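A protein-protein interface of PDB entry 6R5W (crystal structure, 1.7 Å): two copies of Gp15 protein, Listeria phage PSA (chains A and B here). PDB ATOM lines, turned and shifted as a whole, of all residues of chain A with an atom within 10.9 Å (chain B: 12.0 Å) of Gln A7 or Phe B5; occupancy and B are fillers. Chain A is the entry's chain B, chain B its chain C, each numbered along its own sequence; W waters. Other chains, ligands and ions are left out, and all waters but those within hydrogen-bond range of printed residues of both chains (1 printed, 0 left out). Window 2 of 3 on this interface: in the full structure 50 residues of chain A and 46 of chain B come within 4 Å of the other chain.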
ATOM      1  N   ALA A   3      14.050 -22.326  16.859  1.00  0.00           N
ATOM      2  CA  ALA A   3      13.850 -20.880  17.011  1.00  0.00           C
ATOM      3  C   ALA A   3      12.843 -20.569  18.130  1.00  0.00           C
ATOM      4  O   ALA A   3      13.210 -20.078  19.199  1.00  0.00           O
ATOM      5  CB  ALA A   3      13.391 -20.268  15.688  1.00  0.00           C
ATOM      6  N   GLN A   4      11.571 -20.848  17.866  1.00  0.00           N
ATOM      7  CA  GLN A   4      10.516 -20.674  18.850  1.00  0.00           C
ATOM      8  C   GLN A   4      10.381 -21.856  19.812  1.00  0.00           C
ATOM      9  O   GLN A   4       9.440 -21.871  20.613  1.00  0.00           O
ATOM     10  CB  GLN A   4       9.177 -20.428  18.142  1.00  0.00           C
ATOM     11  CG  GLN A   4       8.532 -21.676  17.549  1.00  0.00           C
ATOM     12  CD  GLN A   4       7.818 -21.400  16.236  1.00  0.00           C
ATOM     13  OE1 GLN A   4       8.374 -20.764  15.334  1.00  0.00           O
ATOM     14  NE2 GLN A   4       6.583 -21.872  16.121  1.00  0.00           N
ATOM     15  N   PHE A   5      11.258 -22.853  19.748  1.00  0.00           N
ATOM     16  CA  PHE A   5      11.166 -24.003  20.637  1.00  0.00           C
ATOM     17  C   PHE A   5      12.121 -23.856  21.818  1.00  0.00           C
ATOM     18  O   PHE A   5      13.198 -23.263  21.705  1.00  0.00           O
ATOM     19  CB  PHE A   5      11.475 -25.315  19.911  1.00  0.00           C
ATOM     20  CG  PHE A   5      10.493 -25.644  18.835  1.00  0.00           C
ATOM     21  CD1 PHE A   5       9.135 -25.503  19.065  1.00  0.00           C
ATOM     22  CD2 PHE A   5      10.921 -26.087  17.592  1.00  0.00           C
ATOM     23  CE1 PHE A   5       8.224 -25.793  18.077  1.00  0.00           C
ATOM     24  CE2 PHE A   5      10.006 -26.383  16.599  1.00  0.00           C
ATOM     25  CZ  PHE A   5       8.659 -26.236  16.844  1.00  0.00           C
ATOM     26  N   ALA A   6      11.722 -24.422  22.952  1.00  0.00           N
ATOM     27  CA  ALA A   6      12.528 -24.325  24.159  1.00  0.00           C
ATOM     28  C   ALA A   6      13.631 -25.374  24.136  1.00  0.00           C
ATOM     29  O   ALA A   6      13.413 -26.530  23.765  1.00  0.00           O
ATOM     30  CB  ALA A   6      11.659 -24.488  25.407  1.00  0.00           C
ATOM     31  N   GLN A   7      14.813 -24.971  24.568  1.00  0.00           N
ATOM     32  CA  GLN A   7      15.963 -25.859  24.597  1.00  0.00           C
ATOM     33  C   GLN A   7      15.916 -26.814  25.786  1.00  0.00           C
ATOM     34  O   GLN A   7      15.606 -26.438  26.925  1.00  0.00           O
ATOM     35  CB  GLN A   7      17.259 -25.041  24.589  1.00  0.00           C
ATOM     36  CG  GLN A   7      17.515 -24.292  23.262  1.00  0.00           C
ATOM     37  CD  GLN A   7      17.836 -25.257  22.105  1.00  0.00           C
ATOM     38  OE1 GLN A   7      18.704 -26.130  22.238  1.00  0.00           O
ATOM     39  NE2 GLN A   7      17.148 -25.096  20.977  1.00  0.00           N
ATOM     40  N   LYS A   8      16.230 -28.075  25.503  1.00  0.00           N
ATOM     41  CA  LYS A   8      16.248 -29.094  26.542  1.00  0.00           C
ATOM     42  C   LYS A   8      17.222 -28.754  27.664  1.00  0.00           C
ATOM     43  O   LYS A   8      16.961 -29.077  28.828  1.00  0.00           O
ATOM     44  CB  LYS A   8      16.616 -30.433  25.903  1.00  0.00           C
ATOM     45  CG  LYS A   8      16.941 -31.518  26.860  1.00  0.00           C
ATOM     46  CD  LYS A   8      17.147 -32.863  26.117  1.00  0.00           C
ATOM     47  CE  LYS A   8      15.921 -33.512  25.524  1.00  0.00           C
ATOM     48  NZ  LYS A   8      15.292 -32.783  24.388  1.00  0.00           N
ATOM     49  N   THR A   9      18.345 -28.105  27.360  1.00  0.00           N
ATOM     50  CA  THR A   9      19.284 -27.735  28.414  1.00  0.00           C
ATOM     51  C   THR A   9      18.653 -26.742  29.391  1.00  0.00           C
ATOM     52  O   THR A   9      18.941 -26.774  30.600  1.00  0.00           O
ATOM     53  CB  THR A   9      20.562 -27.126  27.825  1.00  0.00           C
ATOM     54  OG1 THR A   9      20.256 -25.871  27.202  1.00  0.00           O
ATOM     55  CG2 THR A   9      21.228 -28.072  26.821  1.00  0.00           C
ATOM     56  N   VAL A  10      17.829 -25.820  28.871  1.00  0.00           N
ATOM     57  CA  VAL A  10      17.217 -24.796  29.714  1.00  0.00           C
ATOM     58  C   VAL A  10      16.142 -25.418  30.596  1.00  0.00           C
ATOM     59  O   VAL A  10      16.118 -25.210  31.814  1.00  0.00           O
ATOM     60  CB  VAL A  10      16.627 -23.663  28.852  1.00  0.00           C
ATOM     61  CG1 VAL A  10      15.926 -22.641  29.730  1.00  0.00           C
ATOM     62  CG2 VAL A  10      17.719 -23.011  28.009  1.00  0.00           C
ATOM     63  N   LEU A  11      15.270 -26.234  30.003  1.00  0.00           N
ATOM     64  CA  LEU A  11      14.285 -26.960  30.806  1.00  0.00           C
ATOM     65  C   LEU A  11      14.959 -27.832  31.859  1.00  0.00           C
ATOM     66  O   LEU A  11      14.527 -27.860  33.020  1.00  0.00           O
ATOM     67  CB  LEU A  11      13.389 -27.796  29.915  1.00  0.00           C
ATOM     68  CG  LEU A  11      12.418 -28.686  30.688  1.00  0.00           C
ATOM     69  CD1 LEU A  11      11.571 -27.763  31.589  1.00  0.00           C
ATOM     70  CD2 LEU A  11      11.520 -29.436  29.759  1.00  0.00           C
ATOM     71  N   ASP A  12      16.044 -28.530  31.495  1.00  0.00           N
ATOM     72  CA  ASP A  12      16.684 -29.417  32.455  1.00  0.00           C
ATOM     73  C   ASP A  12      17.299 -28.653  33.620  1.00  0.00           C
ATOM     74  O   ASP A  12      17.229 -29.125  34.765  1.00  0.00           O
ATOM     75  CB  ASP A  12      17.763 -30.294  31.790  1.00  0.00           C
ATOM     76  CG  ASP A  12      18.165 -31.495  32.666  1.00  0.00           C
ATOM     77  OD1 ASP A  12      17.358 -32.460  32.783  1.00  0.00           O
ATOM     78  OD2 ASP A  12      19.287 -31.493  33.253  1.00  0.00           O
ATOM     79  N   GLU A  13      17.989 -27.525  33.367  1.00  0.00           N
ATOM     80  CA  GLU A  13      18.573 -26.808  34.496  1.00  0.00           C
ATOM     81  C   GLU A  13      17.458 -26.324  35.441  1.00  0.00           C
ATOM     82  O   GLU A  13      17.607 -26.361  36.665  1.00  0.00           O
ATOM     83  CB  GLU A  13      19.437 -25.626  34.054  1.00  0.00           C
ATOM     84  CG  GLU A  13      19.634 -24.595  35.196  1.00  0.00           C
ATOM     85  CD  GLU A  13      20.805 -23.640  35.002  1.00  0.00           C
ATOM     86  OE1 GLU A  13      21.006 -22.771  35.900  1.00  0.00           O
ATOM     87  OE2 GLU A  13      21.524 -23.736  33.970  1.00  0.00           O
ATOM     88  N   HIS A  14      16.329 -25.891  34.883  1.00  0.00           N
ATOM     89  CA  HIS A  14      15.243 -25.395  35.720  1.00  0.00           C
ATOM     90  C   HIS A  14      14.686 -26.496  36.613  1.00  0.00           C
ATOM     91  O   HIS A  14      14.586 -26.328  37.835  1.00  0.00           O
ATOM     92  CB  HIS A  14      14.131 -24.802  34.866  1.00  0.00           C
ATOM     93  CG  HIS A  14      12.972 -24.319  35.681  1.00  0.00           C
ATOM     94  ND1 HIS A  14      13.022 -23.146  36.414  1.00  0.00           N
ATOM     95  CD2 HIS A  14      11.738 -24.852  35.889  1.00  0.00           C
ATOM     96  CE1 HIS A  14      11.863 -22.984  37.039  1.00  0.00           C
ATOM     97  NE2 HIS A  14      11.074 -24.004  36.744  1.00  0.00           N
ATOM     98  N   VAL A  15      14.366 -27.651  36.018  1.00  0.00           N
ATOM     99  CA  VAL A  15      13.776 -28.768  36.748  1.00  0.00           C
ATOM    100  C   VAL A  15      14.689 -29.288  37.826  1.00  0.00           C
ATOM    101  O   VAL A  15      14.212 -29.767  38.859  1.00  0.00           O
ATOM    102  CB  VAL A  15      13.343 -29.852  35.745  1.00  0.00           C
ATOM    103  CG1 VAL A  15      13.179 -31.179  36.450  1.00  0.00           C
ATOM    104  CG2 VAL A  15      12.060 -29.389  35.023  1.00  0.00           C
ATOM    105  N   ALA B   3      15.398 -33.290  19.267  1.00  0.00           N
ATOM    106  CA  ALA B   3      16.761 -33.698  19.564  1.00  0.00           C
ATOM    107  C   ALA B   3      17.343 -32.746  20.631  1.00  0.00           C
ATOM    108  O   ALA B   3      17.494 -33.125  21.796  1.00  0.00           O
ATOM    109  CB  ALA B   3      17.601 -33.693  18.306  1.00  0.00           C
ATOM    110  N   GLN B   4      17.700 -31.520  20.232  1.00  0.00           N
ATOM    111  CA  GLN B   4      18.136 -30.516  21.197  1.00  0.00           C
ATOM    112  C   GLN B   4      16.961 -29.759  21.826  1.00  0.00           C
ATOM    113  O   GLN B   4      17.175 -28.983  22.761  1.00  0.00           O
ATOM    114  CB  GLN B   4      19.125 -29.531  20.541  1.00  0.00           C
ATOM    115  CG  GLN B   4      18.523 -28.463  19.628  1.00  0.00           C
ATOM    116  CD  GLN B   4      18.755 -28.751  18.152  1.00  0.00           C
ATOM    117  OE1 GLN B   4      18.910 -29.913  17.754  1.00  0.00           O
ATOM    118  NE2 GLN B   4      18.770 -27.704  17.335  1.00  0.00           N
ATOM    119  N   PHE B   5      15.736 -29.984  21.359  1.00  0.00           N
ATOM    120  CA  PHE B   5      14.575 -29.251  21.831  1.00  0.00           C
ATOM    121  C   PHE B   5      13.866 -30.017  22.952  1.00  0.00           C
ATOM    122  O   PHE B   5      13.875 -31.250  23.008  1.00  0.00           O
ATOM    123  CB  PHE B   5      13.595 -29.005  20.682  1.00  0.00           C
ATOM    124  CG  PHE B   5      14.128 -28.128  19.576  1.00  0.00           C
ATOM    125  CD1 PHE B   5      14.790 -26.941  19.852  1.00  0.00           C
ATOM    126  CD2 PHE B   5      13.954 -28.496  18.249  1.00  0.00           C
ATOM    127  CE1 PHE B   5      15.258 -26.134  18.823  1.00  0.00           C
ATOM    128  CE2 PHE B   5      14.420 -27.695  17.217  1.00  0.00           C
ATOM    129  CZ  PHE B   5      15.074 -26.516  17.507  1.00  0.00           C
ATOM    130  N   ALA B   6      13.231 -29.261  23.844  1.00  0.00           N
ATOM    131  CA  ALA B   6      12.556 -29.833  25.000  1.00  0.00           C
ATOM    132  C   ALA B   6      11.209 -30.414  24.597  1.00  0.00           C
ATOM    133  O   ALA B   6      10.496 -29.853  23.769  1.00  0.00           O
ATOM    134  CB  ALA B   6      12.368 -28.757  26.076  1.00  0.00           C
ATOM    135  N   GLN B   7      10.865 -31.544  25.198  1.00  0.00           N
ATOM    136  CA  GLN B   7       9.595 -32.193  24.910  1.00  0.00           C
ATOM    137  C   GLN B   7       8.434 -31.487  25.620  1.00  0.00           C
ATOM    138  O   GLN B   7       8.501 -31.236  26.827  1.00  0.00           O
ATOM    139  CB  GLN B   7       9.659 -33.652  25.366  1.00  0.00           C
ATOM    140  CG  GLN B   7      10.736 -34.463  24.671  1.00  0.00           C
ATOM    141  CD  GLN B   7      10.506 -34.605  23.168  1.00  0.00           C
ATOM    142  OE1 GLN B   7       9.421 -34.986  22.718  1.00  0.00           O
ATOM    143  NE2 GLN B   7      11.530 -34.276  22.383  1.00  0.00           N
ATOM    144  N   LYS B   8       7.352 -31.214  24.883  1.00  0.00           N
ATOM    145  CA  LYS B   8       6.170 -30.601  25.484  1.00  0.00           C
ATOM    146  C   LYS B   8       5.571 -31.451  26.602  1.00  0.00           C
ATOM    147  O   LYS B   8       5.010 -30.896  27.548  1.00  0.00           O
ATOM    148  CB  LYS B   8       5.146 -30.279  24.389  1.00  0.00           C
ATOM    149  CG  LYS B   8       3.676 -30.103  24.819  1.00  0.00           C
ATOM    150  CD  LYS B   8       2.892 -29.265  23.787  1.00  0.00           C
ATOM    151  CE  LYS B   8       1.433 -28.973  24.175  1.00  0.00           C
ATOM    152  NZ  LYS B   8       1.180 -28.361  25.499  1.00  0.00           N
ATOM    153  N   THR B   9       5.658 -32.781  26.524  1.00  0.00           N
ATOM    154  CA  THR B   9       5.097 -33.592  27.601  1.00  0.00           C
ATOM    155  C   THR B   9       5.868 -33.385  28.903  1.00  0.00           C
ATOM    156  O   THR B   9       5.280 -33.415  29.994  1.00  0.00           O
ATOM    157  CB  THR B   9       5.071 -35.075  27.230  1.00  0.00           C
ATOM    158  OG1 THR B   9       6.405 -35.602  27.190  1.00  0.00           O
ATOM    159  CG2 THR B   9       4.380 -35.282  25.869  1.00  0.00           C
ATOM    160  N   VAL B  10       7.195 -33.217  28.816  1.00  0.00           N
ATOM    161  CA  VAL B  10       8.000 -33.061  30.027  1.00  0.00           C
ATOM    162  C   VAL B  10       7.803 -31.681  30.643  1.00  0.00           C
ATOM    163  O   VAL B  10       7.760 -31.553  31.868  1.00  0.00           O
ATOM    164  CB  VAL B  10       9.484 -33.334  29.758  1.00  0.00           C
ATOM    165  CG1 VAL B  10      10.288 -33.069  31.014  1.00  0.00           C
ATOM    166  CG2 VAL B  10       9.680 -34.758  29.299  1.00  0.00           C
ATOM    167  N   LEU B  11       7.777 -30.626  29.820  1.00  0.00           N
ATOM    168  CA  LEU B  11       7.436 -29.298  30.322  1.00  0.00           C
ATOM    169  C   LEU B  11       6.048 -29.301  30.963  1.00  0.00           C
ATOM    170  O   LEU B  11       5.855 -28.775  32.070  1.00  0.00           O
ATOM    171  CB  LEU B  11       7.487 -28.266  29.188  1.00  0.00           C
ATOM    172  CG  LEU B  11       7.026 -26.858  29.565  1.00  0.00           C
ATOM    173  CD1 LEU B  11       7.894 -26.302  30.708  1.00  0.00           C
ATOM    174  CD2 LEU B  11       7.061 -25.904  28.371  1.00  0.00           C
ATOM    175  N   ASP B  12       5.076 -29.920  30.293  1.00  0.00           N
ATOM    176  CA  ASP B  12       3.703 -29.911  30.782  1.00  0.00           C
ATOM    177  C   ASP B  12       3.599 -30.631  32.112  1.00  0.00           C
ATOM    178  O   ASP B  12       2.934 -30.140  33.030  1.00  0.00           O
ATOM    179  CB  ASP B  12       2.764 -30.533  29.750  1.00  0.00           C
ATOM    180  CG  ASP B  12       2.355 -29.545  28.661  1.00  0.00           C
ATOM    181  OD1 ASP B  12       2.858 -28.400  28.658  1.00  0.00           O
ATOM    182  OD2 ASP B  12       1.531 -29.917  27.802  1.00  0.00           O
ATOM    183  N   HIS B  14       5.941 -30.952  34.424  1.00  0.00           N
ATOM    184  CA  HIS B  14       6.545 -30.138  35.464  1.00  0.00           C
ATOM    185  C   HIS B  14       5.623 -28.994  35.847  1.00  0.00           C
ATOM    186  O   HIS B  14       5.392 -28.751  37.038  1.00  0.00           O
ATOM    187  CB  HIS B  14       7.874 -29.583  35.013  1.00  0.00           C
ATOM    188  CG  HIS B  14       8.534 -28.727  36.046  1.00  0.00           C
ATOM    189  ND1 HIS B  14       9.232 -29.268  37.099  1.00  0.00           N
ATOM    190  CD2 HIS B  14       8.583 -27.385  36.211  1.00  0.00           C
ATOM    191  CE1 HIS B  14       9.733 -28.301  37.841  1.00  0.00           C
ATOM    192  NE2 HIS B  14       9.357 -27.149  37.320  1.00  0.00           N
HETATM  193  O   HOH W   1      19.121 -28.449  24.332  1.00  0.00           O
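Among the printed residues, pairs that only touch across the chains: Gln A7 with Phe B5 (3.0 Å), Val A15 with His B14 (3.5 Å), Ala A6 with Phe B5 (3.5 Å), His A14 with His B14 (3.6 Å), Lys A8 with Ala B6 (3.6 Å), Phe A5 with Phe B5 (3.7 Å), Leu A11 with Ala B6 (3.8 Å) and Leu A11 with Leu B11 (3.9 Å).
Of the 13 printed residues of chain A, 7 touch a printed residue of chain B. Printed residues of chain A that touch a printed residue of chain B: Phe A5, Ala A6, Gln A7, Lys A8, Leu A11, His A14 and Val A15. Hydrophobic or aromatic side chains of chain A within 4 Å of the printed part of chain B: Phe A5, Leu A11, His A14 and Val A15. Along chain A the printed residues that touch a printed residue of chain B span positions 5 to 15. Along chain B the printed residues that touch a printed residue of chain A span positions 3 to 14. Among the printed residues, no Asp or Glu carboxylate lies within 4 Å of a Lys or Arg side-chain nitrogen of the other chain.
The backbone NH (N) of Ala B6 lies within hydrogen-bond range of the backbone carbonyl oxygen (O) of Ala A6 (2.7 Å). The backbone carbonyl oxygen (O) of Gln B4 is in hydrogen-bond range of the backbone NH (N) of Lys A8, 3.0 Å away. OE1 of Gln A7 sits close to O of Gln B4. The side-chain amino group (NZ) of Lys A8 lies within hydrogen-bond range of the backbone carbonyl oxygen (O) of Ala B3 (3.4 Å). NZ of Lys A8 lies within hydrogen-bond range of O of Phe B5, 2.5 Å away.
Gln A7 touches just these residues of chain B: Gln B4 and Phe B5. Of chain A, only Phe A5, Ala A6, Gln A7 and Lys A8 come within 4 Å of Phe B5. No residue of chain B comes within 4 Å of Ala A3. Ala A6 touches just these residues of chain B: Phe B5 (3.5 Å) and Ala B6 (2.7 Å). Lys A8 touches just these residues of chain B: Ala B3, Gln B4, Phe B5 and Ala B6. No residue of chain A comes within 4 Å of Gln B7. Of the printed residues of chain B, His A14 touches His B14 (3.6 Å). Of the printed residues of chain B, Val A15 touches His B14 (3.5 Å). Printed residues of chain A within 4 Å of His B14: His A14 and Val A15. Of the printed residues of chain A, Leu B11 touches Leu A11 (3.9 Å). Lys B8 touches none of the printed residues of chain A. Thr B9 touches none of the printed residues of chain A. The nearest residue of chain B that does not touch Gln A7 is Ala B6 (4.1 Å). The nearest printed residue of chain A that does not touch His B14 is Leu A11 (5.4 Å).
Phe B5 touches its own counterpart, Phe A5. Ala A6 touches Phe B5, but with the chains exchanged Phe A5 does not touch Ala B6 (5.8 Å). Gln A7 touches Gln B4, but with the chains exchanged Gln A4 does not touch Gln B7 (10.8 Å). Gln A7 touches Phe B5, but with the chains exchanged Phe A5 does not touch Gln B7 (8.2 Å). Of the 13 pairs that touch across the chains among the printed residues, 4 have their exchanged pair printed and touching as well.
Water W1 lies within hydrogen-bond range of O of Gln B4 (2.6 Å), N of Lys A8 (3.1 Å), N of Thr A9 (3.1 Å) and OE1 of Gln A7 (3.2 Å).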
